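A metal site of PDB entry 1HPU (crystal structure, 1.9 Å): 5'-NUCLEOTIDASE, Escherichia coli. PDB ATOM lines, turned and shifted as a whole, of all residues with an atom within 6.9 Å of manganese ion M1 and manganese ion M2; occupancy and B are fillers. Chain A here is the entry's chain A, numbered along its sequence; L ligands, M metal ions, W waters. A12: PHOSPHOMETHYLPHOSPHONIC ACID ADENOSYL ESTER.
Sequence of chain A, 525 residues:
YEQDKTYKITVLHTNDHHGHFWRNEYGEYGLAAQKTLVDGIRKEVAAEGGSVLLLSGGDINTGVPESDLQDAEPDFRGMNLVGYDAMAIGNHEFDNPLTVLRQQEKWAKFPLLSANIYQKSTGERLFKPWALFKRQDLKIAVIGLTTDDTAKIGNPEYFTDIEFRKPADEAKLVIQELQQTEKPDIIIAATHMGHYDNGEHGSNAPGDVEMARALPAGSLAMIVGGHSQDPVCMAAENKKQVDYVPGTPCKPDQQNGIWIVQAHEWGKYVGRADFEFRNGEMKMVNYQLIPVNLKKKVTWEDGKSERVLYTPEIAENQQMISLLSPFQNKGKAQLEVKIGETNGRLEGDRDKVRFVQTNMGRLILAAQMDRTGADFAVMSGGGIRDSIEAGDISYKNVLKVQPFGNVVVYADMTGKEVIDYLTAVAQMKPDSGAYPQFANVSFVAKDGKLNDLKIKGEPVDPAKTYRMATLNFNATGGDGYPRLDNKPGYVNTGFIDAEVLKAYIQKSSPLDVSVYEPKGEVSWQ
NH2 of Arg 385 lies within salt-bridge range of O3B of the ligand (3.0 Å).
An oxygen (O3B) of the ligand sits at hydrogen-bond distance from a ring nitrogen (NE2) of His 92.
OD1 of Asp 59 lies within hydrogen-bond range of N of His 92 (2.9 Å).
The backbone NH (N) of His 227 lies within hydrogen-bond range of the side-chain carboxylate (OD2) of Asp 16, 2.7 Å away.
The backbone NH (N) of Thr 147 lies within hydrogen-bond range of the backbone carbonyl oxygen (O) of His 192.
A ring nitrogen (ND1) of His 18 is in hydrogen-bond range of the backbone carbonyl oxygen (O) of Asn 61.
The backbone NH (N) of His 17 sits at hydrogen-bond distance from the backbone carbonyl oxygen (O) of Asp 59.
The backbone NH of Trp 266 lies within hydrogen-bond range of the backbone carbonyl oxygen of Asp 16.
The side-chain amide nitrogen (ND2) of Asn 15 is in hydrogen-bond range of the side-chain carboxylate (OD2) of Asp 16 (2.7 Å).
The side-chain amide nitrogen of Gln 229 is in hydrogen-bond range of the side-chain carboxylate of Glu 265, 2.7 Å away.
Four residues have an atom within 4 Å of manganese ion M2: Asp 59, Asn 91, His 192 and His 227.
Manganese ion M1 is bound by OD1 of Asp 16 (2.1 Å), water W1 (2.2 Å), NE2 of His 18 (2.3 Å), OE1 of Gln 229 (2.3 Å) and OD2 of Asp 59 (2.4 Å).
O1B of the ligand is bound to manganese ion M2 (2.2 Å).
Manganese ion M2 is bound by OD1 of Asn 91.
Manganese ion M2 is bound by a ring nitrogen (NE2) of His 192 (2.2 Å).
Water W1 binds manganese ion M2 (2.3 Å).
A ring nitrogen (ND1) of His 227 binds manganese ion M2 (2.3 Å).
The side-chain carboxylate (OD2) of Asp 59 binds manganese ion M2 (2.4 Å).
Manganese ion M2 has six donor atoms within binding distance.
Water W1 lies within hydrogen-bond range of O2B of the ligand (2.5 Å) and O of His 227 (2.7 Å).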
ATOM      1  N   ASN A  15      17.351 -11.146 -30.297  1.00  0.00           N
ATOM      2  CA  ASN A  15      18.632 -10.898 -29.645  1.00  0.00           C
ATOM      3  C   ASN A  15      18.935  -9.422 -29.680  1.00  0.00           C
ATOM      4  O   ASN A  15      18.349  -8.682 -30.468  1.00  0.00           O
ATOM      5  CB  ASN A  15      19.755 -11.610 -30.396  1.00  0.00           C
ATOM      6  CG  ASN A  15      19.784 -11.231 -31.851  1.00  0.00           C
ATOM      7  OD1 ASN A  15      19.004 -11.736 -32.633  1.00  0.00           O
ATOM      8  ND2 ASN A  15      20.700 -10.317 -32.235  1.00  0.00           N
ATOM      9  N   ASP A  16      19.878  -9.007 -28.826  1.00  0.00           N
ATOM     10  CA  ASP A  16      20.334  -7.622 -28.841  1.00  0.00           C
ATOM     11  C   ASP A  16      19.207  -6.589 -28.738  1.00  0.00           C
ATOM     12  O   ASP A  16      19.169  -5.594 -29.485  1.00  0.00           O
ATOM     13  CB  ASP A  16      21.171  -7.428 -30.097  1.00  0.00           C
ATOM     14  CG  ASP A  16      22.481  -8.251 -30.034  1.00  0.00           C
ATOM     15  OD1 ASP A  16      23.447  -7.726 -29.451  1.00  0.00           O
ATOM     16  OD2 ASP A  16      22.512  -9.408 -30.502  1.00  0.00           O
ATOM     17  N   HIS A  17      18.316  -6.871 -27.796  1.00  0.00           N
ATOM     18  CA  HIS A  17      17.151  -6.046 -27.464  1.00  0.00           C
ATOM     19  C   HIS A  17      17.585  -4.617 -27.093  1.00  0.00           C
ATOM     20  O   HIS A  17      16.969  -3.626 -27.506  1.00  0.00           O
ATOM     21  CB  HIS A  17      16.422  -6.719 -26.307  1.00  0.00           C
ATOM     22  CG  HIS A  17      15.244  -5.946 -25.819  1.00  0.00           C
ATOM     23  ND1 HIS A  17      14.025  -5.983 -26.468  1.00  0.00           N
ATOM     24  CD2 HIS A  17      15.108  -5.086 -24.791  1.00  0.00           C
ATOM     25  CE1 HIS A  17      13.184  -5.166 -25.847  1.00  0.00           C
ATOM     26  NE2 HIS A  17      13.812  -4.613 -24.830  1.00  0.00           N
ATOM     27  N   HIS A  18      18.639  -4.509 -26.297  1.00  0.00           N
ATOM     28  CA  HIS A  18      19.183  -3.201 -25.949  1.00  0.00           C
ATOM     29  C   HIS A  18      18.213  -2.110 -25.473  1.00  0.00           C
ATOM     30  O   HIS A  18      18.235  -0.998 -25.997  1.00  0.00           O
ATOM     31  CB  HIS A  18      20.009  -2.659 -27.119  1.00  0.00           C
ATOM     32  CG  HIS A  18      21.358  -3.328 -27.245  1.00  0.00           C
ATOM     33  ND1 HIS A  18      22.210  -3.454 -26.165  1.00  0.00           N
ATOM     34  CD2 HIS A  18      21.972  -3.929 -28.294  1.00  0.00           C
ATOM     35  CE1 HIS A  18      23.303  -4.110 -26.547  1.00  0.00           C
ATOM     36  NE2 HIS A  18      23.180  -4.402 -27.825  1.00  0.00           N
ATOM     37  N   GLY A  58      20.640 -12.564 -25.944  1.00  0.00           N
ATOM     38  CA  GLY A  58      21.254 -11.644 -25.009  1.00  0.00           C
ATOM     39  C   GLY A  58      21.455 -10.186 -25.367  1.00  0.00           C
ATOM     40  O   GLY A  58      21.128  -9.741 -26.465  1.00  0.00           O
ATOM     41  N   ASP A  59      22.076  -9.448 -24.454  1.00  0.00           N
ATOM     42  CA  ASP A  59      22.306  -8.011 -24.614  1.00  0.00           C
ATOM     43  C   ASP A  59      20.922  -7.321 -24.566  1.00  0.00           C
ATOM     44  O   ASP A  59      20.520  -6.636 -25.500  1.00  0.00           O
ATOM     45  CB  ASP A  59      22.999  -7.637 -25.942  1.00  0.00           C
ATOM     46  CG  ASP A  59      24.525  -7.406 -25.785  1.00  0.00           C
ATOM     47  OD1 ASP A  59      25.138  -7.785 -24.759  1.00  0.00           O
ATOM     48  OD2 ASP A  59      25.118  -6.847 -26.719  1.00  0.00           O
ATOM     49  N   ASN A  61      20.332  -5.410 -21.930  1.00  0.00           N
ATOM     50  CA  ASN A  61      20.754  -4.130 -21.351  1.00  0.00           C
ATOM     51  C   ASN A  61      21.359  -3.096 -22.266  1.00  0.00           C
ATOM     52  O   ASN A  61      22.081  -3.415 -23.205  1.00  0.00           O
ATOM     53  CB  ASN A  61      21.822  -4.371 -20.271  1.00  0.00           C
ATOM     54  CG  ASN A  61      21.245  -4.890 -18.984  1.00  0.00           C
ATOM     55  OD1 ASN A  61      20.724  -4.107 -18.161  1.00  0.00           O
ATOM     56  ND2 ASN A  61      21.320  -6.203 -18.779  1.00  0.00           N
ATOM     57  N   GLY A  90      24.702 -11.733 -22.496  1.00  0.00           N
ATOM     58  CA  GLY A  90      25.462 -10.969 -23.473  1.00  0.00           C
ATOM     59  C   GLY A  90      26.485 -10.145 -22.712  1.00  0.00           C
ATOM     60  O   GLY A  90      26.443 -10.117 -21.483  1.00  0.00           O
ATOM     61  N   ASN A  91      27.398  -9.471 -23.409  1.00  0.00           N
ATOM     62  CA  ASN A  91      28.404  -8.692 -22.713  1.00  0.00           C
ATOM     63  C   ASN A  91      27.808  -7.514 -21.998  1.00  0.00           C
ATOM     64  O   ASN A  91      28.290  -7.128 -20.914  1.00  0.00           O
ATOM     65  CB  ASN A  91      29.521  -8.236 -23.654  1.00  0.00           C
ATOM     66  CG  ASN A  91      29.001  -7.555 -24.918  1.00  0.00           C
ATOM     67  OD1 ASN A  91      28.308  -8.172 -25.707  1.00  0.00           O
ATOM     68  ND2 ASN A  91      29.368  -6.300 -25.111  1.00  0.00           N
ATOM     69  N   HIS A  92      26.757  -6.929 -22.573  1.00  0.00           N
ATOM     70  CA  HIS A  92      26.144  -5.788 -21.951  1.00  0.00           C
ATOM     71  C   HIS A  92      25.411  -6.049 -20.655  1.00  0.00           C
ATOM     72  O   HIS A  92      25.017  -5.099 -19.975  1.00  0.00           O
ATOM     73  CB  HIS A  92      25.276  -5.019 -22.957  1.00  0.00           C
ATOM     74  CG  HIS A  92      26.073  -4.194 -23.902  1.00  0.00           C
ATOM     75  ND1 HIS A  92      26.575  -2.960 -23.568  1.00  0.00           N
ATOM     76  CD2 HIS A  92      26.574  -4.482 -25.130  1.00  0.00           C
ATOM     77  CE1 HIS A  92      27.358  -2.520 -24.538  1.00  0.00           C
ATOM     78  NE2 HIS A  92      27.370  -3.428 -25.504  1.00  0.00           N
ATOM     79  N   THR A 147      30.374 -14.305 -25.458  1.00  0.00           N
ATOM     80  CA  THR A 147      31.647 -14.000 -26.102  1.00  0.00           C
ATOM     81  C   THR A 147      32.743 -13.716 -25.084  1.00  0.00           C
ATOM     82  O   THR A 147      32.529 -13.000 -24.106  1.00  0.00           O
ATOM     83  CB  THR A 147      31.580 -12.766 -27.000  1.00  0.00           C
ATOM     84  OG1 THR A 147      32.899 -12.480 -27.479  1.00  0.00           O
ATOM     85  CG2 THR A 147      31.077 -11.553 -26.251  1.00  0.00           C
ATOM     86  N   ILE A 153      36.313  -5.759 -23.927  1.00  0.00           N
ATOM     87  CA  ILE A 153      35.602  -4.554 -24.392  1.00  0.00           C
ATOM     88  C   ILE A 153      34.653  -3.970 -23.355  1.00  0.00           C
ATOM     89  O   ILE A 153      33.921  -3.016 -23.630  1.00  0.00           O
ATOM     90  CB  ILE A 153      34.739  -4.863 -25.635  1.00  0.00           C
ATOM     91  CG1 ILE A 153      33.639  -5.869 -25.266  1.00  0.00           C
ATOM     92  CG2 ILE A 153      35.612  -5.358 -26.768  1.00  0.00           C
ATOM     93  CD1 ILE A 153      32.629  -6.167 -26.360  1.00  0.00           C
ATOM     94  N   HIS A 192      25.979 -15.417 -27.369  1.00  0.00           N
ATOM     95  CA  HIS A 192      26.199 -14.013 -27.628  1.00  0.00           C
ATOM     96  C   HIS A 192      27.642 -13.965 -28.101  1.00  0.00           C
ATOM     97  O   HIS A 192      28.536 -13.522 -27.371  1.00  0.00           O
ATOM     98  CB  HIS A 192      26.034 -13.177 -26.364  1.00  0.00           C
ATOM     99  CG  HIS A 192      25.908 -11.716 -26.670  1.00  0.00           C
ATOM    100  ND1 HIS A 192      24.762 -11.174 -27.199  1.00  0.00           N
ATOM    101  CD2 HIS A 192      26.841 -10.733 -26.672  1.00  0.00           C
ATOM    102  CE1 HIS A 192      24.976  -9.916 -27.516  1.00  0.00           C
ATOM    103  NE2 HIS A 192      26.229  -9.614 -27.212  1.00  0.00           N
ATOM    104  N   GLY A 226      23.670 -13.762 -31.589  1.00  0.00           N
ATOM    105  CA  GLY A 226      23.538 -12.356 -31.329  1.00  0.00           C
ATOM    106  C   GLY A 226      24.892 -11.685 -31.372  1.00  0.00           C
ATOM    107  O   GLY A 226      25.821 -12.195 -32.029  1.00  0.00           O
ATOM    108  N   HIS A 227      24.980 -10.538 -30.696  1.00  0.00           N
ATOM    109  CA  HIS A 227      26.201  -9.733 -30.601  1.00  0.00           C
ATOM    110  C   HIS A 227      26.645  -8.972 -31.866  1.00  0.00           C
ATOM    111  O   HIS A 227      26.878  -7.765 -31.807  1.00  0.00           O
ATOM    112  CB  HIS A 227      27.347 -10.649 -30.108  1.00  0.00           C
ATOM    113  CG  HIS A 227      28.604  -9.914 -29.780  1.00  0.00           C
ATOM    114  ND1 HIS A 227      28.647  -8.844 -28.921  1.00  0.00           N
ATOM    115  CD2 HIS A 227      29.886 -10.103 -30.198  1.00  0.00           C
ATOM    116  CE1 HIS A 227      29.876  -8.394 -28.815  1.00  0.00           C
ATOM    117  NE2 HIS A 227      30.655  -9.149 -29.578  1.00  0.00           N
ATOM    118  N   SER A 228      26.773  -9.640 -33.011  1.00  0.00           N
ATOM    119  CA  SER A 228      27.201  -8.927 -34.213  1.00  0.00           C
ATOM    120  C   SER A 228      26.068  -8.067 -34.747  1.00  0.00           C
ATOM    121  O   SER A 228      26.290  -7.169 -35.555  1.00  0.00           O
ATOM    122  CB  SER A 228      27.654  -9.928 -35.294  1.00  0.00           C
ATOM    123  OG  SER A 228      26.691 -10.956 -35.520  1.00  0.00           O
ATOM    124  N   GLN A 229      24.857  -8.354 -34.268  1.00  0.00           N
ATOM    125  CA  GLN A 229      23.633  -7.667 -34.656  1.00  0.00           C
ATOM    126  C   GLN A 229      23.392  -7.688 -36.143  1.00  0.00           C
ATOM    127  O   GLN A 229      23.447  -6.666 -36.827  1.00  0.00           O
ATOM    128  CB  GLN A 229      23.625  -6.235 -34.094  1.00  0.00           C
ATOM    129  CG  GLN A 229      23.428  -6.308 -32.578  1.00  0.00           C
ATOM    130  CD  GLN A 229      23.586  -4.960 -31.863  1.00  0.00           C
ATOM    131  OE1 GLN A 229      24.291  -4.862 -30.848  1.00  0.00           O
ATOM    132  NE2 GLN A 229      22.954  -3.932 -32.387  1.00  0.00           N
ATOM    133  N   HIS A 264      18.968  -9.834 -36.044  1.00  0.00           N
ATOM    134  CA  HIS A 264      19.421  -8.463 -36.076  1.00  0.00           C
ATOM    135  C   HIS A 264      19.493  -7.773 -34.708  1.00  0.00           C
ATOM    136  O   HIS A 264      20.489  -7.943 -34.013  1.00  0.00           O
ATOM    137  CB  HIS A 264      18.571  -7.641 -37.063  1.00  0.00           C
ATOM    138  CG  HIS A 264      19.230  -6.372 -37.518  1.00  0.00           C
ATOM    139  ND1 HIS A 264      18.746  -5.604 -38.561  1.00  0.00           N
ATOM    140  CD2 HIS A 264      20.353  -5.757 -37.083  1.00  0.00           C
ATOM    141  CE1 HIS A 264      19.545  -4.577 -38.755  1.00  0.00           C
ATOM    142  NE2 HIS A 264      20.533  -4.643 -37.876  1.00  0.00           N
ATOM    143  N   GLU A 265      18.467  -7.021 -34.299  1.00  0.00           N
ATOM    144  CA  GLU A 265      18.575  -6.305 -33.026  1.00  0.00           C
ATOM    145  C   GLU A 265      17.269  -5.589 -32.638  1.00  0.00           C
ATOM    146  O   GLU A 265      16.368  -5.465 -33.466  1.00  0.00           O
ATOM    147  CB  GLU A 265      19.610  -5.196 -33.207  1.00  0.00           C
ATOM    148  CG  GLU A 265      19.104  -4.091 -34.204  1.00  0.00           C
ATOM    149  CD  GLU A 265      20.179  -3.169 -34.759  1.00  0.00           C
ATOM    150  OE1 GLU A 265      21.397  -3.364 -34.487  1.00  0.00           O
ATOM    151  OE2 GLU A 265      19.800  -2.233 -35.513  1.00  0.00           O
ATOM    152  N   TRP A 266      17.206  -5.141 -31.392  1.00  0.00           N
ATOM    153  CA  TRP A 266      16.114  -4.293 -30.894  1.00  0.00           C
ATOM    154  C   TRP A 266      14.669  -4.762 -31.075  1.00  0.00           C
ATOM    155  O   TRP A 266      13.761  -3.923 -31.157  1.00  0.00           O
ATOM    156  CB  TRP A 266      16.209  -2.911 -31.564  1.00  0.00           C
ATOM    157  CG  TRP A 266      17.552  -2.208 -31.516  1.00  0.00           C
ATOM    158  CD1 TRP A 266      18.662  -2.569 -30.815  1.00  0.00           C
ATOM    159  CD2 TRP A 266      17.888  -0.994 -32.208  1.00  0.00           C
ATOM    160  NE1 TRP A 266      19.683  -1.650 -31.015  1.00  0.00           N
ATOM    161  CE2 TRP A 266      19.230  -0.679 -31.859  1.00  0.00           C
ATOM    162  CE3 TRP A 266      17.183  -0.136 -33.060  1.00  0.00           C
ATOM    163  CZ2 TRP A 266      19.880   0.459 -32.361  1.00  0.00           C
ATOM    164  CZ3 TRP A 266      17.833   1.002 -33.562  1.00  0.00           C
ATOM    165  CH2 TRP A 266      19.180   1.285 -33.201  1.00  0.00           C
ATOM    166  N   ARG A 385      27.592   6.565 -28.535  1.00  0.00           N
ATOM    167  CA  ARG A 385      26.545   5.738 -29.106  1.00  0.00           C
ATOM    168  C   ARG A 385      25.376   6.420 -29.821  1.00  0.00           C
ATOM    169  O   ARG A 385      24.398   5.774 -30.168  1.00  0.00           O
ATOM    170  CB  ARG A 385      26.020   4.799 -28.002  1.00  0.00           C
ATOM    171  CG  ARG A 385      27.042   3.739 -27.521  1.00  0.00           C
ATOM    172  CD  ARG A 385      27.593   2.938 -28.712  1.00  0.00           C
ATOM    173  NE  ARG A 385      28.460   1.815 -28.349  1.00  0.00           N
ATOM    174  CZ  ARG A 385      28.059   0.567 -28.210  1.00  0.00           C
ATOM    175  NH1 ARG A 385      26.781   0.249 -28.393  1.00  0.00           N
ATOM    176  NH2 ARG A 385      28.934  -0.385 -27.927  1.00  0.00           N
HETATM  177  PB  A12 L   1      28.727  -4.627 -28.532  1.00  0.00           P
HETATM  178  O1B A12 L   1      28.413  -5.816 -27.676  1.00  0.00           O
HETATM  179  O2B A12 L   1      27.662  -4.419 -29.565  1.00  0.00           O
HETATM  180  O3B A12 L   1      28.813  -3.391 -27.717  1.00  0.00           O
HETATM  181  PA  A12 L   1      30.809  -3.459 -30.328  1.00  0.00           P
HETATM  182  O1A A12 L   1      29.718  -3.026 -31.247  1.00  0.00           O
HETATM  183  O2A A12 L   1      32.033  -3.824 -31.079  1.00  0.00           O
HETATM  184  C3A A12 L   1      30.261  -4.852 -29.381  1.00  0.00           C
HETATM  185  O5' A12 L   1      31.121  -2.246 -29.339  1.00  0.00           O
HETATM  186  C5' A12 L   1      32.091  -2.443 -28.334  1.00  0.00           C
HETATM  187  C4' A12 L   1      32.711  -1.132 -27.930  1.00  0.00           C
HETATM  188  O4' A12 L   1      31.730  -0.320 -27.224  1.00  0.00           O
HETATM  189  C3' A12 L   1      33.858  -1.301 -26.961  1.00  0.00           C
HETATM  190  O3' A12 L   1      35.044  -1.540 -27.708  1.00  0.00           O
HETATM  191  C2' A12 L   1      33.858   0.034 -26.226  1.00  0.00           C
HETATM  192  O2' A12 L   1      34.452   1.047 -26.991  1.00  0.00           O
HETATM  193  C1' A12 L   1      32.349   0.332 -26.121  1.00  0.00           C
HETATM  194  N9  A12 L   1      31.741  -0.160 -24.881  1.00  0.00           N
HETATM  195  C8  A12 L   1      30.961  -1.275 -24.733  1.00  0.00           C
HETATM  196  N7  A12 L   1      30.545  -1.483 -23.501  1.00  0.00           N
HETATM  197  C5  A12 L   1      31.087  -0.413 -22.800  1.00  0.00           C
HETATM  198  C6  A12 L   1      30.990  -0.045 -21.452  1.00  0.00           C
HETATM  199  N6  A12 L   1      30.296  -0.718 -20.547  1.00  0.00           N
HETATM  200  N1  A12 L   1      31.654   1.070 -21.057  1.00  0.00           N
HETATM  201  C2  A12 L   1      32.337   1.762 -21.975  1.00  0.00           C
HETATM  202  N3  A12 L   1      32.480   1.528 -23.285  1.00  0.00           N
HETATM  203  C4  A12 L   1      31.828   0.407 -23.633  1.00  0.00           C
HETATM  204 MN    MN M   1      24.420  -6.012 -28.837  1.00  0.00          MN
HETATM  205 MN    MN M   2      27.209  -7.629 -27.540  1.00  0.00          MN
HETATM  206  O   HOH W   1      26.450  -6.566 -29.452  1.00  0.00           O
